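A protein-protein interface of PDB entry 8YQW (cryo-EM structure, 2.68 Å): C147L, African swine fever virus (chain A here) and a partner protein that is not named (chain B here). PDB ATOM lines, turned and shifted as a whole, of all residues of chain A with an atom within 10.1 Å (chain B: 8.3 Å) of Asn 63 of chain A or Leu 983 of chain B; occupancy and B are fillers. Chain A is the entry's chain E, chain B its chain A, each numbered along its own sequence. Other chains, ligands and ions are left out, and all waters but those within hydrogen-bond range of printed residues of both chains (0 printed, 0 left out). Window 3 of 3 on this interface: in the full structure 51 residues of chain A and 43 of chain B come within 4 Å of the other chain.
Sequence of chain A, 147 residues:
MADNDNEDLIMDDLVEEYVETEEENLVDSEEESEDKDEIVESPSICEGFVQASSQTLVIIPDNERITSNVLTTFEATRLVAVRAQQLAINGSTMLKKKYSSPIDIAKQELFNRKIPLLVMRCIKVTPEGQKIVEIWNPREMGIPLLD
Of the 12 printed residues of chain A, 7 touch a printed residue of chain B. Printed residues of chain A that touch a printed residue of chain B: Asp 62, Asn 63, Glu 64, Arg 65, Ile 66, Thr 67 and Trp 136. Hydrophobic or aromatic side chains of chain A that line the printed part of chain B: Trp 136. Printed residues of chain B that touch a printed residue of chain A: Asn 977, Ile 979, Gln 980, Arg 982 and Leu 983. Among the printed residues, 11 pairs touch across the chains.
The backbone NH of Gln 980 of chain B sits at hydrogen-bond distance from the side-chain amide oxygen of Asn 977 of chain B (2.7 Å). The side-chain hydroxyl (OG1) of Thr 985 of chain B lies within hydrogen-bond range of the side-chain amide oxygen (OE1) of Gln 980 of chain B, at 3.1 Å. NH1 of Arg 65 of chain A is in hydrogen-bond range of O of Ile 135 of chain A, at 2.7 Å. The backbone NH (N) of Ile 66 of chain A lies within hydrogen-bond range of the side-chain carboxylate (OE2) of Glu 134 of chain A (2.9 Å). OG1 of Thr 67 of chain A is in hydrogen-bond range of NE1 of Trp 136 of chain A, at 2.7 Å. The side-chain carboxylate (OE1) of Glu 134 of chain A is in hydrogen-bond range of the indole nitrogen (NE1) of Trp 136 of chain A (3.2 Å).
ND2 of Asn 977 of chain B sits at hydrogen-bond distance from O of Arg 65 of chain A (2.6 Å). The backbone carbonyl oxygen (O) of Ile 66 of chain A sits at hydrogen-bond distance from the side-chain amide nitrogen (ND2) of Asn 977 of chain B, 3.4 Å away. The backbone carbonyl oxygen of Thr 67 of chain A sits at hydrogen-bond distance from the side-chain amide nitrogen of Asn 977 of chain B. The side-chain amide nitrogen (NE2) of Gln 980 of chain B is in hydrogen-bond range of the backbone carbonyl oxygen (O) of Asn 63 of chain A. O of Arg 65 of chain A lies within hydrogen-bond range of NE2 of Gln 980 of chain B, at 2.9 Å. The guanidinium group (NH2) of Arg 982 of chain B sits close to the side-chain amide nitrogen (ND2) of Asn 63 of chain A, at 3.5 Å.
Leu 983 of chain B touches one residue of chain A. Gln 980 of chain B touches three residues of chain A. Printed residues of chain A within 4 Å of Arg 982 of chain B: Asn 63. No residue of chain A comes within 4 Å of Thr 985 of chain B. Of the printed residues of chain B, Ile 66 of chain A touches Asn 977. Printed residues of chain B within 4 Å of Asp 62 of chain A: Ile 979. Printed residues of chain A within 4 Å of Ile 979 of chain B: Asp 62, Arg 65 and Trp 136. Ile 135 of chain A touches none of the printed residues of chain B. Ile 60 of chain A touches none of the printed residues of chain B. The nearest residue of chain B that does not touch Asn 63 of chain A is Ile 979 of chain B (4.1 Å). The nearest residue of chain A that does not touch Leu 983 of chain B is Glu 64 of chain A (5.6 Å).
Asp 62 of chain A touches Ile 979 of chain B (O to CD1, 3.7 Å). Asn 63 of chain A touches Leu 983 of chain B (O to CD1, 3.3 Å). NE2 of Gln 980 of chain B touches C of Glu 64 of chain A, at 3.8 Å. Ile 979 of chain B touches Arg 65 of chain A (CD1 to NH2, 3.7 Å). Ile 979 of chain B touches Trp 136 of chain A.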
ATOM      1  N   ILE A  59     -18.588   6.734   4.411  1.00  0.00           N
ATOM      2  CA  ILE A  59     -17.344   6.998   5.120  1.00  0.00           C
ATOM      3  C   ILE A  59     -17.556   6.694   6.595  1.00  0.00           C
ATOM      4  O   ILE A  59     -18.448   7.261   7.235  1.00  0.00           O
ATOM      5  CB  ILE A  59     -16.888   8.449   4.912  1.00  0.00           C
ATOM      6  CG1 ILE A  59     -16.557   8.685   3.439  1.00  0.00           C
ATOM      7  CG2 ILE A  59     -15.694   8.756   5.785  1.00  0.00           C
ATOM      8  CD1 ILE A  59     -16.354  10.134   3.084  1.00  0.00           C
ATOM      9  N   ILE A  60     -16.749   5.790   7.128  1.00  0.00           N
ATOM     10  CA  ILE A  60     -16.839   5.442   8.549  1.00  0.00           C
ATOM     11  C   ILE A  60     -16.437   6.655   9.382  1.00  0.00           C
ATOM     12  O   ILE A  60     -15.413   7.293   9.082  1.00  0.00           O
ATOM     13  CB  ILE A  60     -15.948   4.239   8.856  1.00  0.00           C
ATOM     14  CG1 ILE A  60     -16.551   2.972   8.254  1.00  0.00           C
ATOM     15  CG2 ILE A  60     -15.761   4.073  10.349  1.00  0.00           C
ATOM     16  CD1 ILE A  60     -15.731   1.733   8.498  1.00  0.00           C
ATOM     17  N   PRO A  61     -17.203   7.024  10.408  1.00  0.00           N
ATOM     18  CA  PRO A  61     -16.820   8.175  11.233  1.00  0.00           C
ATOM     19  C   PRO A  61     -15.456   7.966  11.870  1.00  0.00           C
ATOM     20  O   PRO A  61     -15.052   6.842  12.174  1.00  0.00           O
ATOM     21  CB  PRO A  61     -17.931   8.250  12.287  1.00  0.00           C
ATOM     22  CG  PRO A  61     -18.654   6.951  12.203  1.00  0.00           C
ATOM     23  CD  PRO A  61     -18.506   6.471  10.803  1.00  0.00           C
ATOM     24  N   ASP A  62     -14.740   9.077  12.060  1.00  0.00           N
ATOM     25  CA  ASP A  62     -13.338   9.011  12.461  1.00  0.00           C
ATOM     26  C   ASP A  62     -13.149   8.285  13.787  1.00  0.00           C
ATOM     27  O   ASP A  62     -12.099   7.675  14.012  1.00  0.00           O
ATOM     28  CB  ASP A  62     -12.755  10.421  12.540  1.00  0.00           C
ATOM     29  CG  ASP A  62     -12.358  10.962  11.182  1.00  0.00           C
ATOM     30  OD1 ASP A  62     -12.771  10.372  10.162  1.00  0.00           O
ATOM     31  OD2 ASP A  62     -11.630  11.975  11.131  1.00  0.00           O
ATOM     32  N   ASN A  63     -14.143   8.330  14.671  1.00  0.00           N
ATOM     33  CA  ASN A  63     -14.022   7.678  15.968  1.00  0.00           C
ATOM     34  C   ASN A  63     -14.371   6.197  15.927  1.00  0.00           C
ATOM     35  O   ASN A  63     -14.281   5.531  16.962  1.00  0.00           O
ATOM     36  CB  ASN A  63     -14.906   8.386  16.994  1.00  0.00           C
ATOM     37  CG  ASN A  63     -14.483   9.820  17.227  1.00  0.00           C
ATOM     38  OD1 ASN A  63     -15.206  10.756  16.886  1.00  0.00           O
ATOM     39  ND2 ASN A  63     -13.302  10.002  17.805  1.00  0.00           N
ATOM     40  N   GLU A  64     -14.760   5.669  14.767  1.00  0.00           N
ATOM     41  CA  GLU A  64     -15.125   4.265  14.629  1.00  0.00           C
ATOM     42  C   GLU A  64     -14.189   3.520  13.686  1.00  0.00           C
ATOM     43  O   GLU A  64     -14.464   2.373  13.325  1.00  0.00           O
ATOM     44  CB  GLU A  64     -16.569   4.137  14.149  1.00  0.00           C
ATOM     45  CG  GLU A  64     -17.585   4.688  15.125  1.00  0.00           C
ATOM     46  CD  GLU A  64     -19.008   4.447  14.679  1.00  0.00           C
ATOM     47  OE1 GLU A  64     -19.203   3.954  13.549  1.00  0.00           O
ATOM     48  OE2 GLU A  64     -19.934   4.753  15.457  1.00  0.00           O
ATOM     49  N   ARG A  65     -13.092   4.149  13.276  1.00  0.00           N
ATOM     50  CA  ARG A  65     -12.154   3.523  12.356  1.00  0.00           C
ATOM     51  C   ARG A  65     -11.379   2.410  13.049  1.00  0.00           C
ATOM     52  O   ARG A  65     -10.957   2.549  14.200  1.00  0.00           O
ATOM     53  CB  ARG A  65     -11.193   4.564  11.789  1.00  0.00           C
ATOM     54  CG  ARG A  65     -11.837   5.522  10.810  1.00  0.00           C
ATOM     55  CD  ARG A  65     -10.827   6.489  10.235  1.00  0.00           C
ATOM     56  NE  ARG A  65     -10.339   7.425  11.239  1.00  0.00           N
ATOM     57  CZ  ARG A  65      -9.549   8.456  10.977  1.00  0.00           C
ATOM     58  NH1 ARG A  65      -9.146   8.722   9.747  1.00  0.00           N
ATOM     59  NH2 ARG A  65      -9.155   9.239  11.976  1.00  0.00           N
ATOM     60  N   ILE A  66     -11.191   1.303  12.333  1.00  0.00           N
ATOM     61  CA  ILE A  66     -10.565   0.117  12.889  1.00  0.00           C
ATOM     62  C   ILE A  66      -9.155  -0.112  12.351  1.00  0.00           C
ATOM     63  O   ILE A  66      -8.327  -0.701  13.055  1.00  0.00           O
ATOM     64  CB  ILE A  66     -11.456  -1.120  12.639  1.00  0.00           C
ATOM     65  CG1 ILE A  66     -12.824  -0.922  13.283  1.00  0.00           C
ATOM     66  CG2 ILE A  66     -10.827  -2.386  13.178  1.00  0.00           C
ATOM     67  CD1 ILE A  66     -12.757  -0.745  14.778  1.00  0.00           C
ATOM     68  N   THR A  67      -8.848   0.349  11.145  1.00  0.00           N
ATOM     69  CA  THR A  67      -7.529   0.119  10.581  1.00  0.00           C
ATOM     70  C   THR A  67      -6.485   0.966  11.308  1.00  0.00           C
ATOM     71  O   THR A  67      -6.804   1.891  12.057  1.00  0.00           O
ATOM     72  CB  THR A  67      -7.531   0.420   9.085  1.00  0.00           C
ATOM     73  OG1 THR A  67      -8.046   1.736   8.863  1.00  0.00           O
ATOM     74  CG2 THR A  67      -8.403  -0.575   8.352  1.00  0.00           C
ATOM     75  N   GLU A 134     -12.808   3.719   4.771  1.00  0.00           N
ATOM     76  CA  GLU A 134     -12.201   4.559   5.795  1.00  0.00           C
ATOM     77  C   GLU A 134     -11.258   5.540   5.118  1.00  0.00           C
ATOM     78  O   GLU A 134     -10.450   5.145   4.273  1.00  0.00           O
ATOM     79  CB  GLU A 134     -11.439   3.728   6.829  1.00  0.00           C
ATOM     80  CG  GLU A 134     -12.316   2.836   7.677  1.00  0.00           C
ATOM     81  CD  GLU A 134     -11.542   2.136   8.768  1.00  0.00           C
ATOM     82  OE1 GLU A 134     -10.313   2.324   8.838  1.00  0.00           O
ATOM     83  OE2 GLU A 134     -12.161   1.392   9.554  1.00  0.00           O
ATOM     84  N   ILE A 135     -11.364   6.810   5.486  1.00  0.00           N
ATOM     85  CA  ILE A 135     -10.512   7.859   4.940  1.00  0.00           C
ATOM     86  C   ILE A 135      -9.480   8.217   5.997  1.00  0.00           C
ATOM     87  O   ILE A 135      -9.833   8.531   7.139  1.00  0.00           O
ATOM     88  CB  ILE A 135     -11.327   9.090   4.519  1.00  0.00           C
ATOM     89  CG1 ILE A 135     -12.495   8.683   3.623  1.00  0.00           C
ATOM     90  CG2 ILE A 135     -10.441  10.087   3.797  1.00  0.00           C
ATOM     91  CD1 ILE A 135     -12.090   8.285   2.233  1.00  0.00           C
ATOM     92  N   TRP A 136      -8.208   8.167   5.621  1.00  0.00           N
ATOM     93  CA  TRP A 136      -7.107   8.428   6.534  1.00  0.00           C
ATOM     94  C   TRP A 136      -6.282   9.594   6.013  1.00  0.00           C
ATOM     95  O   TRP A 136      -5.967   9.656   4.823  1.00  0.00           O
ATOM     96  CB  TRP A 136      -6.235   7.185   6.707  1.00  0.00           C
ATOM     97  CG  TRP A 136      -6.804   6.206   7.677  1.00  0.00           C
ATOM     98  CD1 TRP A 136      -7.564   5.118   7.386  1.00  0.00           C
ATOM     99  CD2 TRP A 136      -6.670   6.233   9.102  1.00  0.00           C
ATOM    100  NE1 TRP A 136      -7.911   4.461   8.538  1.00  0.00           N
ATOM    101  CE2 TRP A 136      -7.374   5.127   9.607  1.00  0.00           C
ATOM    102  CE3 TRP A 136      -6.020   7.086   9.999  1.00  0.00           C
ATOM    103  CZ2 TRP A 136      -7.445   4.848  10.966  1.00  0.00           C
ATOM    104  CZ3 TRP A 136      -6.096   6.809  11.344  1.00  0.00           C
ATOM    105  CH2 TRP A 136      -6.801   5.700  11.816  1.00  0.00           C
ATOM    106  N   LYS B 969      -2.325  -4.841  29.311  1.00  0.00           N
ATOM    107  CA  LYS B 969      -3.769  -4.847  29.108  1.00  0.00           C
ATOM    108  C   LYS B 969      -4.144  -4.223  27.769  1.00  0.00           C
ATOM    109  O   LYS B 969      -5.070  -4.689  27.098  1.00  0.00           O
ATOM    110  CB  LYS B 969      -4.451  -4.116  30.265  1.00  0.00           C
ATOM    111  CG  LYS B 969      -5.956  -4.278  30.329  1.00  0.00           C
ATOM    112  CD  LYS B 969      -6.667  -3.084  29.712  1.00  0.00           C
ATOM    113  CE  LYS B 969      -8.175  -3.225  29.811  1.00  0.00           C
ATOM    114  NZ  LYS B 969      -8.875  -2.109  29.119  1.00  0.00           N
ATOM    115  N   TYR B 973      -4.306  -3.595  21.289  1.00  0.00           N
ATOM    116  CA  TYR B 973      -4.641  -2.416  20.500  1.00  0.00           C
ATOM    117  C   TYR B 973      -3.572  -2.073  19.475  1.00  0.00           C
ATOM    118  O   TYR B 973      -3.812  -1.212  18.623  1.00  0.00           O
ATOM    119  CB  TYR B 973      -4.888  -1.220  21.413  1.00  0.00           C
ATOM    120  CG  TYR B 973      -6.234  -1.258  22.093  1.00  0.00           C
ATOM    121  CD1 TYR B 973      -7.403  -1.261  21.352  1.00  0.00           C
ATOM    122  CD2 TYR B 973      -6.336  -1.294  23.473  1.00  0.00           C
ATOM    123  CE1 TYR B 973      -8.633  -1.299  21.964  1.00  0.00           C
ATOM    124  CE2 TYR B 973      -7.562  -1.331  24.094  1.00  0.00           C
ATOM    125  CZ  TYR B 973      -8.707  -1.333  23.334  1.00  0.00           C
ATOM    126  OH  TYR B 973      -9.933  -1.372  23.950  1.00  0.00           O
ATOM    127  N   ASN B 977      -5.646   0.294  16.346  1.00  0.00           N
ATOM    128  CA  ASN B 977      -5.183   1.672  16.180  1.00  0.00           C
ATOM    129  C   ASN B 977      -5.161   2.316  17.560  1.00  0.00           C
ATOM    130  O   ASN B 977      -5.571   1.712  18.555  1.00  0.00           O
ATOM    131  CB  ASN B 977      -6.027   2.510  15.204  1.00  0.00           C
ATOM    132  CG  ASN B 977      -7.494   2.569  15.575  1.00  0.00           C
ATOM    133  OD1 ASN B 977      -7.857   2.836  16.715  1.00  0.00           O
ATOM    134  ND2 ASN B 977      -8.351   2.341  14.593  1.00  0.00           N
ATOM    135  N   ASN B 978      -4.675   3.555  17.609  1.00  0.00           N
ATOM    136  CA  ASN B 978      -4.680   4.326  18.845  1.00  0.00           C
ATOM    137  C   ASN B 978      -6.019   4.994  19.129  1.00  0.00           C
ATOM    138  O   ASN B 978      -6.225   5.475  20.247  1.00  0.00           O
ATOM    139  CB  ASN B 978      -3.577   5.386  18.807  1.00  0.00           C
ATOM    140  CG  ASN B 978      -3.802   6.429  17.729  1.00  0.00           C
ATOM    141  OD1 ASN B 978      -4.664   6.275  16.866  1.00  0.00           O
ATOM    142  ND2 ASN B 978      -3.022   7.500  17.776  1.00  0.00           N
ATOM    143  N   ILE B 979      -6.923   5.053  18.150  1.00  0.00           N
ATOM    144  CA  ILE B 979      -8.233   5.655  18.379  1.00  0.00           C
ATOM    145  C   ILE B 979      -9.075   4.767  19.282  1.00  0.00           C
ATOM    146  O   ILE B 979      -9.731   5.246  20.214  1.00  0.00           O
ATOM    147  CB  ILE B 979      -8.942   5.930  17.040  1.00  0.00           C
ATOM    148  CG1 ILE B 979      -8.082   6.824  16.149  1.00  0.00           C
ATOM    149  CG2 ILE B 979     -10.300   6.558  17.276  1.00  0.00           C
ATOM    150  CD1 ILE B 979      -8.521   6.836  14.709  1.00  0.00           C
ATOM    151  N   GLN B 980      -9.076   3.459  19.017  1.00  0.00           N
ATOM    152  CA  GLN B 980      -9.866   2.545  19.832  1.00  0.00           C
ATOM    153  C   GLN B 980      -9.230   2.318  21.195  1.00  0.00           C
ATOM    154  O   GLN B 980      -9.937   2.031  22.166  1.00  0.00           O
ATOM    155  CB  GLN B 980     -10.051   1.214  19.106  1.00  0.00           C
ATOM    156  CG  GLN B 980     -10.623   1.341  17.708  1.00  0.00           C
ATOM    157  CD  GLN B 980     -11.961   2.046  17.680  1.00  0.00           C
ATOM    158  OE1 GLN B 980     -12.861   1.724  18.449  1.00  0.00           O
ATOM    159  NE2 GLN B 980     -12.097   3.014  16.788  1.00  0.00           N
ATOM    160  N   GLU B 981      -7.903   2.430  21.285  1.00  0.00           N
ATOM    161  CA  GLU B 981      -7.240   2.317  22.579  1.00  0.00           C
ATOM    162  C   GLU B 981      -7.666   3.442  23.510  1.00  0.00           C
ATOM    163  O   GLU B 981      -7.880   3.220  24.707  1.00  0.00           O
ATOM    164  CB  GLU B 981      -5.726   2.321  22.397  1.00  0.00           C
ATOM    165  CG  GLU B 981      -4.955   2.087  23.680  1.00  0.00           C
ATOM    166  CD  GLU B 981      -3.459   2.121  23.471  1.00  0.00           C
ATOM    167  OE1 GLU B 981      -3.023   2.337  22.321  1.00  0.00           O
ATOM    168  OE2 GLU B 981      -2.717   1.929  24.456  1.00  0.00           O
ATOM    169  N   ARG B 982      -7.783   4.661  22.981  1.00  0.00           N
ATOM    170  CA  ARG B 982      -8.258   5.779  23.788  1.00  0.00           C
ATOM    171  C   ARG B 982      -9.702   5.570  24.226  1.00  0.00           C
ATOM    172  O   ARG B 982     -10.065   5.886  25.364  1.00  0.00           O
ATOM    173  CB  ARG B 982      -8.114   7.081  23.003  1.00  0.00           C
ATOM    174  CG  ARG B 982      -8.445   8.328  23.794  1.00  0.00           C
ATOM    175  CD  ARG B 982      -8.471   9.553  22.896  1.00  0.00           C
ATOM    176  NE  ARG B 982      -9.599   9.533  21.974  1.00  0.00           N
ATOM    177  CZ  ARG B 982      -9.485   9.492  20.654  1.00  0.00           C
ATOM    178  NH1 ARG B 982      -8.303   9.469  20.063  1.00  0.00           N
ATOM    179  NH2 ARG B 982     -10.586   9.473  19.908  1.00  0.00           N
ATOM    180  N   LEU B 983     -10.539   5.041  23.336  1.00  0.00           N
ATOM    181  CA  LEU B 983     -11.938   4.789  23.644  1.00  0.00           C
ATOM    182  C   LEU B 983     -12.149   3.525  24.465  1.00  0.00           C
ATOM    183  O   LEU B 983     -13.242   3.342  25.012  1.00  0.00           O
ATOM    184  CB  LEU B 983     -12.750   4.696  22.352  1.00  0.00           C
ATOM    185  CG  LEU B 983     -12.828   5.959  21.499  1.00  0.00           C
ATOM    186  CD1 LEU B 983     -13.604   5.686  20.227  1.00  0.00           C
ATOM    187  CD2 LEU B 983     -13.466   7.088  22.284  1.00  0.00           C
ATOM    188  N   GLN B 984     -11.140   2.659  24.557  1.00  0.00           N
ATOM    189  CA  GLN B 984     -11.225   1.410  25.317  1.00  0.00           C
ATOM    190  C   GLN B 984     -12.387   0.541  24.842  1.00  0.00           C
ATOM    191  O   GLN B 984     -13.123  -0.036  25.643  1.00  0.00           O
ATOM    192  CB  GLN B 984     -11.325   1.680  26.818  1.00  0.00           C
ATOM    193  CG  GLN B 984     -10.066   2.271  27.419  1.00  0.00           C
ATOM    194  CD  GLN B 984      -8.865   1.368  27.240  1.00  0.00           C
ATOM    195  OE1 GLN B 984      -8.924   0.175  27.529  1.00  0.00           O
ATOM    196  NE2 GLN B 984      -7.768   1.932  26.755  1.00  0.00           N
ATOM    197  N   THR B 985     -12.555   0.450  23.527  1.00  0.00           N
ATOM    198  CA  THR B 985     -13.576  -0.419  22.969  1.00  0.00           C
ATOM    199  C   THR B 985     -13.161  -1.883  23.128  1.00  0.00           C
ATOM    200  O   THR B 985     -11.971  -2.189  23.234  1.00  0.00           O
ATOM    201  CB  THR B 985     -13.807  -0.092  21.496  1.00  0.00           C
ATOM    202  OG1 THR B 985     -12.582  -0.240  20.774  1.00  0.00           O
ATOM    203  CG2 THR B 985     -14.308   1.331  21.347  1.00  0.00           C
ATOM    204  N   PRO B 986     -14.126  -2.805  23.167  1.00  0.00           N
ATOM    205  CA  PRO B 986     -13.785  -4.215  23.393  1.00  0.00           C
ATOM    206  C   PRO B 986     -12.872  -4.765  22.308  1.00  0.00           C
ATOM    207  O   PRO B 986     -12.975  -4.404  21.135  1.00  0.00           O
ATOM    208  CB  PRO B 986     -15.149  -4.915  23.389  1.00  0.00           C
ATOM    209  CG  PRO B 986     -16.075  -3.958  22.728  1.00  0.00           C
ATOM    210  CD  PRO B 986     -15.581  -2.607  23.109  1.00  0.00           C
